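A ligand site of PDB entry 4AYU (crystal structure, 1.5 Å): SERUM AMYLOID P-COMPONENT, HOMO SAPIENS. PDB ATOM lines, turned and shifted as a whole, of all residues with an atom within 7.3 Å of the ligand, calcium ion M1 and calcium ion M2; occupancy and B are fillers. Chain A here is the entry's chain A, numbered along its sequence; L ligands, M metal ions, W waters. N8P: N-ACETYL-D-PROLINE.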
ATOM      1  N   ALA A  46     -10.095 -20.779 -20.790  1.00  0.00           N
ATOM      2  CA  ALA A  46      -8.838 -21.507 -20.844  1.00  0.00           C
ATOM      3  C   ALA A  46      -8.761 -22.528 -19.722  1.00  0.00           C
ATOM      4  O   ALA A  46      -9.376 -22.373 -18.659  1.00  0.00           O
ATOM      5  CB  ALA A  46      -7.664 -20.529 -20.746  1.00  0.00           C
ATOM      6  N   TYR A  47      -7.997 -23.579 -19.943  1.00  0.00           N
ATOM      7  CA  TYR A  47      -7.796 -24.595 -18.930  1.00  0.00           C
ATOM      8  C   TYR A  47      -6.572 -25.441 -19.191  1.00  0.00           C
ATOM      9  O   TYR A  47      -6.162 -25.612 -20.324  1.00  0.00           O
ATOM     10  CB  TYR A  47      -9.046 -25.485 -18.790  1.00  0.00           C
ATOM     11  CG  TYR A  47      -9.563 -26.151 -20.051  1.00  0.00           C
ATOM     12  CD1 TYR A  47      -9.069 -27.362 -20.478  1.00  0.00           C
ATOM     13  CD2 TYR A  47     -10.608 -25.584 -20.760  1.00  0.00           C
ATOM     14  CE1 TYR A  47      -9.582 -27.990 -21.608  1.00  0.00           C
ATOM     15  CE2 TYR A  47     -11.121 -26.204 -21.885  1.00  0.00           C
ATOM     16  CZ  TYR A  47     -10.620 -27.410 -22.300  1.00  0.00           C
ATOM     17  OH  TYR A  47     -11.134 -28.038 -23.430  1.00  0.00           O
ATOM     18  N   SER A  48      -6.010 -25.992 -18.124  1.00  0.00           N
ATOM     19  CA  SER A  48      -4.914 -26.919 -18.206  1.00  0.00           C
ATOM     20  C   SER A  48      -5.401 -28.350 -18.485  1.00  0.00           C
ATOM     21  O   SER A  48      -6.320 -28.855 -17.805  1.00  0.00           O
ATOM     22  CB  SER A  48      -4.122 -26.918 -16.892  1.00  0.00           C
ATOM     23  OG  SER A  48      -3.071 -27.853 -16.953  1.00  0.00           O
ATOM     24  N   SER A  51      -0.440 -30.989 -16.584  1.00  0.00           N
ATOM     25  CA  SER A  51       0.472 -30.070 -15.895  1.00  0.00           C
ATOM     26  C   SER A  51       1.605 -30.877 -15.253  1.00  0.00           C
ATOM     27  O   SER A  51       1.352 -31.706 -14.383  1.00  0.00           O
ATOM     28  CB  SER A  51      -0.307 -29.293 -14.834  1.00  0.00           C
ATOM     29  OG  SER A  51       0.530 -28.528 -13.974  1.00  0.00           O
ATOM     30  N   ASN A  53       5.227 -30.163 -13.420  1.00  0.00           N
ATOM     31  CA  ASN A  53       6.120 -29.202 -12.775  1.00  0.00           C
ATOM     32  C   ASN A  53       7.226 -29.967 -12.063  1.00  0.00           C
ATOM     33  O   ASN A  53       7.050 -31.102 -11.633  1.00  0.00           O
ATOM     34  CB  ASN A  53       5.354 -28.363 -11.743  1.00  0.00           C
ATOM     35  CG  ASN A  53       4.712 -27.117 -12.331  1.00  0.00           C
ATOM     36  OD1 ASN A  53       4.534 -27.015 -13.546  1.00  0.00           O
ATOM     37  ND2 ASN A  53       4.356 -26.172 -11.456  1.00  0.00           N
ATOM     38  N   ASP A  58       8.127 -23.925 -12.519  1.00  0.00           N
ATOM     39  CA  ASP A  58       6.747 -23.882 -12.997  1.00  0.00           C
ATOM     40  C   ASP A  58       6.712 -24.092 -14.503  1.00  0.00           C
ATOM     41  O   ASP A  58       7.669 -23.793 -15.199  1.00  0.00           O
ATOM     42  CB  ASP A  58       6.115 -22.541 -12.642  1.00  0.00           C
ATOM     43  CG  ASP A  58       4.631 -22.506 -12.894  1.00  0.00           C
ATOM     44  OD1 ASP A  58       3.989 -23.577 -12.730  1.00  0.00           O
ATOM     45  OD2 ASP A  58       4.080 -21.429 -13.243  1.00  0.00           O
ATOM     46  N   ASN A  59       5.603 -24.639 -14.992  1.00  0.00           N
ATOM     47  CA  ASN A  59       5.367 -24.763 -16.424  1.00  0.00           C
ATOM     48  C   ASN A  59       6.505 -25.468 -17.131  1.00  0.00           C
ATOM     49  O   ASN A  59       6.941 -25.063 -18.211  1.00  0.00           O
ATOM     50  CB  ASN A  59       5.123 -23.397 -17.056  1.00  0.00           C
ATOM     51  CG  ASN A  59       3.955 -22.687 -16.409  1.00  0.00           C
ATOM     52  OD1 ASN A  59       3.172 -23.312 -15.693  1.00  0.00           O
ATOM     53  ND2 ASN A  59       3.826 -21.396 -16.651  1.00  0.00           N
ATOM     54  N   GLU A  60       6.980 -26.540 -16.526  1.00  0.00           N
ATOM     55  CA  GLU A  60       8.115 -27.265 -17.064  1.00  0.00           C
ATOM     56  C   GLU A  60       7.690 -28.061 -18.302  1.00  0.00           C
ATOM     57  O   GLU A  60       8.430 -28.125 -19.290  1.00  0.00           O
ATOM     58  CB  GLU A  60       8.736 -28.149 -15.983  1.00  0.00           C
ATOM     59  CG  GLU A  60       9.968 -28.905 -16.431  1.00  0.00           C
ATOM     60  CD  GLU A  60      11.159 -28.009 -16.743  1.00  0.00           C
ATOM     61  OE1 GLU A  60      11.102 -26.815 -16.433  1.00  0.00           O
ATOM     62  OE2 GLU A  60      12.133 -28.510 -17.309  1.00  0.00           O
ATOM     63  N   LEU A  62       3.678 -28.330 -19.999  1.00  0.00           N
ATOM     64  CA  LEU A  62       2.275 -28.017 -19.775  1.00  0.00           C
ATOM     65  C   LEU A  62       1.512 -27.976 -21.085  1.00  0.00           C
ATOM     66  O   LEU A  62       1.899 -27.288 -22.040  1.00  0.00           O
ATOM     67  CB  LEU A  62       2.127 -26.670 -19.059  1.00  0.00           C
ATOM     68  CG  LEU A  62       0.746 -26.015 -19.036  1.00  0.00           C
ATOM     69  CD1 LEU A  62      -0.234 -26.803 -18.168  1.00  0.00           C
ATOM     70  CD2 LEU A  62       0.846 -24.559 -18.528  1.00  0.00           C
ATOM     71  N   TYR A  64      -1.961 -26.809 -22.500  1.00  0.00           N
ATOM     72  CA  TYR A  64      -2.893 -25.796 -22.032  1.00  0.00           C
ATOM     73  C   TYR A  64      -3.812 -25.401 -23.178  1.00  0.00           C
ATOM     74  O   TYR A  64      -3.340 -25.091 -24.282  1.00  0.00           O
ATOM     75  CB  TYR A  64      -2.124 -24.573 -21.562  1.00  0.00           C
ATOM     76  CG  TYR A  64      -2.919 -23.517 -20.821  1.00  0.00           C
ATOM     77  CD1 TYR A  64      -3.333 -23.732 -19.518  1.00  0.00           C
ATOM     78  CD2 TYR A  64      -3.182 -22.280 -21.391  1.00  0.00           C
ATOM     79  CE1 TYR A  64      -4.018 -22.769 -18.821  1.00  0.00           C
ATOM     80  CE2 TYR A  64      -3.886 -21.301 -20.697  1.00  0.00           C
ATOM     81  CZ  TYR A  64      -4.290 -21.552 -19.413  1.00  0.00           C
ATOM     82  OH  TYR A  64      -4.965 -20.596 -18.669  1.00  0.00           O
ATOM     83  N   GLU A  66      -6.114 -22.740 -24.764  1.00  0.00           N
ATOM     84  CA  GLU A  66      -6.296 -21.301 -24.637  1.00  0.00           C
ATOM     85  C   GLU A  66      -7.755 -20.862 -24.822  1.00  0.00           C
ATOM     86  O   GLU A  66      -8.238 -19.930 -24.191  1.00  0.00           O
ATOM     87  CB  GLU A  66      -5.462 -20.572 -25.707  1.00  0.00           C
ATOM     88  CG  GLU A  66      -3.978 -20.900 -25.710  1.00  0.00           C
ATOM     89  CD  GLU A  66      -3.208 -20.246 -24.595  1.00  0.00           C
ATOM     90  OE1 GLU A  66      -3.769 -19.366 -23.901  1.00  0.00           O
ATOM     91  OE2 GLU A  66      -2.029 -20.599 -24.417  1.00  0.00           O
ATOM     92  N   TYR A  74       3.788 -25.685 -23.284  1.00  0.00           N
ATOM     93  CA  TYR A  74       4.916 -25.038 -22.634  1.00  0.00           C
ATOM     94  C   TYR A  74       5.998 -26.080 -22.389  1.00  0.00           C
ATOM     95  O   TYR A  74       5.697 -27.176 -21.940  1.00  0.00           O
ATOM     96  CB  TYR A  74       4.532 -24.431 -21.274  1.00  0.00           C
ATOM     97  CG  TYR A  74       3.601 -23.240 -21.290  1.00  0.00           C
ATOM     98  CD1 TYR A  74       2.274 -23.367 -21.694  1.00  0.00           C
ATOM     99  CD2 TYR A  74       4.026 -21.990 -20.855  1.00  0.00           C
ATOM    100  CE1 TYR A  74       1.421 -22.294 -21.666  1.00  0.00           C
ATOM    101  CE2 TYR A  74       3.174 -20.919 -20.845  1.00  0.00           C
ATOM    102  CZ  TYR A  74       1.878 -21.081 -21.255  1.00  0.00           C
ATOM    103  OH  TYR A  74       1.018 -20.012 -21.240  1.00  0.00           O
ATOM    104  N   LYS A  79       6.575 -21.135 -24.556  1.00  0.00           N
ATOM    105  CA  LYS A  79       5.363 -21.729 -25.123  1.00  0.00           C
ATOM    106  C   LYS A  79       5.275 -21.601 -26.631  1.00  0.00           C
ATOM    107  O   LYS A  79       5.835 -20.669 -27.247  1.00  0.00           O
ATOM    108  CB  LYS A  79       4.099 -21.133 -24.502  1.00  0.00           C
ATOM    109  CG  LYS A  79       3.810 -19.733 -24.948  1.00  0.00           C
ATOM    110  CD  LYS A  79       2.623 -19.097 -24.215  1.00  0.00           C
ATOM    111  CE  LYS A  79       1.313 -19.777 -24.526  1.00  0.00           C
ATOM    112  NZ  LYS A  79       0.132 -19.066 -23.897  1.00  0.00           N
ATOM    113  N   GLU A 136      -3.984 -26.665 -12.945  1.00  0.00           N
ATOM    114  CA  GLU A 136      -2.707 -26.147 -13.407  1.00  0.00           C
ATOM    115  C   GLU A 136      -1.844 -25.842 -12.183  1.00  0.00           C
ATOM    116  O   GLU A 136      -2.258 -25.079 -11.325  1.00  0.00           O
ATOM    117  CB  GLU A 136      -2.953 -24.877 -14.229  1.00  0.00           C
ATOM    118  CG  GLU A 136      -1.871 -24.582 -15.253  1.00  0.00           C
ATOM    119  CD  GLU A 136      -0.622 -23.972 -14.663  1.00  0.00           C
ATOM    120  OE1 GLU A 136      -0.759 -23.089 -13.786  1.00  0.00           O
ATOM    121  OE2 GLU A 136       0.485 -24.376 -15.065  1.00  0.00           O
ATOM    122  N   GLN A 137      -0.673 -26.458 -12.094  1.00  0.00           N
ATOM    123  CA  GLN A 137       0.224 -26.201 -10.951  1.00  0.00           C
ATOM    124  C   GLN A 137       0.949 -24.888 -11.123  1.00  0.00           C
ATOM    125  O   GLN A 137       1.383 -24.591 -12.218  1.00  0.00           O
ATOM    126  CB  GLN A 137       1.280 -27.281 -10.831  1.00  0.00           C
ATOM    127  CG  GLN A 137       0.786 -28.662 -10.535  1.00  0.00           C
ATOM    128  CD  GLN A 137       1.882 -29.701 -10.666  1.00  0.00           C
ATOM    129  OE1 GLN A 137       2.657 -29.937  -9.733  1.00  0.00           O
ATOM    130  NE2 GLN A 137       1.963 -30.317 -11.835  1.00  0.00           N
ATOM    131  N   ASP A 138       1.125 -24.147 -10.035  1.00  0.00           N
ATOM    132  CA  ASP A 138       2.114 -23.055  -9.993  1.00  0.00           C
ATOM    133  C   ASP A 138       3.252 -23.333  -9.023  1.00  0.00           C
ATOM    134  O   ASP A 138       4.201 -22.554  -8.941  1.00  0.00           O
ATOM    135  CB  ASP A 138       1.445 -21.730  -9.662  1.00  0.00           C
ATOM    136  CG  ASP A 138       0.605 -21.199 -10.797  1.00  0.00           C
ATOM    137  OD1 ASP A 138       0.890 -21.534 -11.964  1.00  0.00           O
ATOM    138  OD2 ASP A 138      -0.341 -20.409 -10.537  1.00  0.00           O
ATOM    139  N   SER A 139       3.159 -24.426  -8.272  1.00  0.00           N
ATOM    140  CA  SER A 139       4.233 -24.874  -7.397  1.00  0.00           C
ATOM    141  C   SER A 139       4.507 -26.347  -7.660  1.00  0.00           C
ATOM    142  O   SER A 139       3.924 -26.939  -8.565  1.00  0.00           O
ATOM    143  CB  SER A 139       3.825 -24.676  -5.941  1.00  0.00           C
ATOM    144  OG  SER A 139       2.787 -25.589  -5.612  1.00  0.00           O
ATOM    145  N   GLY A 142       1.202 -28.054  -6.356  1.00  0.00           N
ATOM    146  CA  GLY A 142       0.089 -27.258  -5.881  1.00  0.00           C
ATOM    147  C   GLY A 142      -0.018 -25.875  -6.489  1.00  0.00           C
ATOM    148  O   GLY A 142       0.363 -25.665  -7.643  1.00  0.00           O
ATOM    149  N   LYS A 143      -0.565 -24.950  -5.699  1.00  0.00           N
ATOM    150  CA  LYS A 143      -0.839 -23.570  -6.096  1.00  0.00           C
ATOM    151  C   LYS A 143      -1.676 -23.559  -7.362  1.00  0.00           C
ATOM    152  O   LYS A 143      -1.293 -22.971  -8.384  1.00  0.00           O
ATOM    153  CB  LYS A 143       0.456 -22.754  -6.239  1.00  0.00           C
ATOM    154  CG  LYS A 143       1.128 -22.462  -4.897  1.00  0.00           C
ATOM    155  CD  LYS A 143       0.304 -21.498  -4.058  1.00  0.00           C
ATOM    156  CE  LYS A 143       1.045 -21.118  -2.778  1.00  0.00           C
ATOM    157  NZ  LYS A 143       0.206 -20.295  -1.859  1.00  0.00           N
ATOM    158  N   PHE A 144      -2.841 -24.171  -7.251  1.00  0.00           N
ATOM    159  CA  PHE A 144      -3.804 -24.279  -8.335  1.00  0.00           C
ATOM    160  C   PHE A 144      -4.593 -22.981  -8.479  1.00  0.00           C
ATOM    161  O   PHE A 144      -4.498 -22.070  -7.654  1.00  0.00           O
ATOM    162  CB  PHE A 144      -4.751 -25.452  -8.061  1.00  0.00           C
ATOM    163  CG  PHE A 144      -4.072 -26.779  -7.869  1.00  0.00           C
ATOM    164  CD1 PHE A 144      -2.974 -27.140  -8.630  1.00  0.00           C
ATOM    165  CD2 PHE A 144      -4.535 -27.669  -6.914  1.00  0.00           C
ATOM    166  CE1 PHE A 144      -2.369 -28.360  -8.463  1.00  0.00           C
ATOM    167  CE2 PHE A 144      -3.933 -28.905  -6.740  1.00  0.00           C
ATOM    168  CZ  PHE A 144      -2.845 -29.250  -7.526  1.00  0.00           C
ATOM    169  N   ASP A 145      -5.390 -22.905  -9.551  1.00  0.00           N
ATOM    170  CA  ASP A 145      -6.143 -21.706  -9.905  1.00  0.00           C
ATOM    171  C   ASP A 145      -7.466 -22.164 -10.519  1.00  0.00           C
ATOM    172  O   ASP A 145      -7.485 -22.777 -11.596  1.00  0.00           O
ATOM    173  CB  ASP A 145      -5.320 -20.874 -10.891  1.00  0.00           C
ATOM    174  CG  ASP A 145      -6.039 -19.616 -11.387  1.00  0.00           C
ATOM    175  OD1 ASP A 145      -7.257 -19.447 -11.157  1.00  0.00           O
ATOM    176  OD2 ASP A 145      -5.374 -18.809 -12.050  1.00  0.00           O
ATOM    177  N   GLN A 148      -8.283 -21.930 -14.205  1.00  0.00           N
ATOM    178  CA  GLN A 148      -7.537 -22.794 -15.115  1.00  0.00           C
ATOM    179  C   GLN A 148      -7.881 -24.266 -14.911  1.00  0.00           C
ATOM    180  O   GLN A 148      -7.272 -25.137 -15.551  1.00  0.00           O
ATOM    181  CB  GLN A 148      -6.045 -22.591 -14.928  1.00  0.00           C
ATOM    182  CG  GLN A 148      -5.589 -21.168 -15.190  1.00  0.00           C
ATOM    183  CD  GLN A 148      -4.092 -20.957 -14.957  1.00  0.00           C
ATOM    184  OE1 GLN A 148      -3.546 -21.368 -13.944  1.00  0.00           O
ATOM    185  NE2 GLN A 148      -3.439 -20.314 -15.909  1.00  0.00           N
HETATM  186  C7  N8P L   1      -0.844 -17.741 -17.067  1.00  0.00           C
HETATM  187  O9  N8P L   1      -1.797 -17.125 -17.565  1.00  0.00           O
HETATM  188  C8  N8P L   1       0.029 -17.119 -16.036  1.00  0.00           C
HETATM  189  N   N8P L   1      -0.573 -19.078 -17.474  1.00  0.00           N
HETATM  190  CA  N8P L   1       0.508 -19.883 -16.981  1.00  0.00           C
HETATM  191  CB  N8P L   1       0.550 -21.083 -17.879  1.00  0.00           C
HETATM  192  CG  N8P L   1      -0.820 -21.224 -18.405  1.00  0.00           C
HETATM  193  CD  N8P L   1      -1.334 -19.801 -18.478  1.00  0.00           C
HETATM  194  C   N8P L   1       0.372 -20.306 -15.545  1.00  0.00           C
HETATM  195  O   N8P L   1      -0.735 -20.162 -14.946  1.00  0.00           O
HETATM  196  OXT N8P L   1       1.366 -20.806 -14.954  1.00  0.00           O
HETATM  197 CA    CA M   1      -1.415 -21.004 -12.831  1.00  0.00          CA
HETATM  198 CA    CA M   2       1.835 -22.809 -13.745  1.00  0.00          CA
HETATM  199  O   HOH W   1      -0.205 -18.557 -12.949  1.00  0.00           O
HETATM  200  O   HOH W   2      -2.724 -19.051 -12.265  1.00  0.00           O
HETATM  201  O   HOH W   3      -2.341 -22.396 -11.039  1.00  0.00           O
HETATM  202  O   HOH W   4       2.422 -18.668 -12.486  1.00  0.00           O
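The backbone carbonyl oxygen (O) of Lys 143 lies within hydrogen-bond range of the backbone NH (N) of Asp 138, 3.2 Å away.
The backbone carbonyl oxygen (O) of Gln 137 sits close to the side-chain amide nitrogen (ND2) of Asn 53 (3.5 Å).
O of Ser 139 lies close to OE1 of Gln 137, at 3.5 Å.
The side-chain amide nitrogen of Gln 137 is in hydrogen-bond range of the backbone carbonyl oxygen of Ser 51 (3.0 Å).
The side-chain amide oxygen (OD1) of Asn 53 is in hydrogen-bond range of the backbone NH (N) of Asn 59, 3.0 Å away.
The side-chain carboxylate (OD1) of Asp 58 sits close to the side-chain amide nitrogen (ND2) of Asn 53 (2.9 Å).
The backbone NH (N) of Tyr 74 sits at hydrogen-bond distance from the backbone carbonyl oxygen (O) of Leu 62 (2.8 Å).
OH of Tyr 74 lies within hydrogen-bond range of NZ of Lys 79 (3.0 Å).
Leu 62 touches the ligand.
CZ of Tyr 64 touches CD of the ligand (3.6 Å).
Tyr 74 touches the ligand.
Hydrophobic or aromatic side chains within 4 Å of the ligand: Leu 62, Tyr 64 and Tyr 74.
Of the 22 residues printed, 8 come within 4 Å of the ligand.
The nearest printed residue that does not touch the ligand is Gln 137 (4.7 Å).
Three residues have an atom within 4 Å of calcium ion M1: Glu 136, Asp 138 and Gln 148.
Of the 22 residues printed, 5 come within 4 Å of calcium ion M2.
The nearest printed residue that does not touch calcium ion M2 is Asn 53 (4.8 Å).
Calcium ion M1 is bound by an oxygen (O) of the ligand, the side-chain carboxylate (OE1) of Glu 136, water W2, the side-chain amide oxygen (OE1) of Gln 148, water W3, the side-chain carboxylate (OD1) of Asp 138, the side-chain carboxylate (OD2) of Asp 138 and water W1.
Calcium ion M1 has eight donor atoms within binding distance.
Calcium ion M2 is bound by OD1 of Asp 138 (2.4 Å), OXT of the ligand (2.4 Å), O of Gln 137 (2.4 Å), OD1 of Asn 59 (2.4 Å), OE2 of Glu 136 (2.5 Å), OD1 of Asp 58 (2.5 Å), OE1 of Glu 136 (2.6 Å) and OD2 of Asp 58 (2.7 Å).
Calcium ion M2 has eight donor atoms within binding distance.
Water W3 lies within hydrogen-bond range of O of Glu 136, O of Lys 143 and N of Asp 145.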
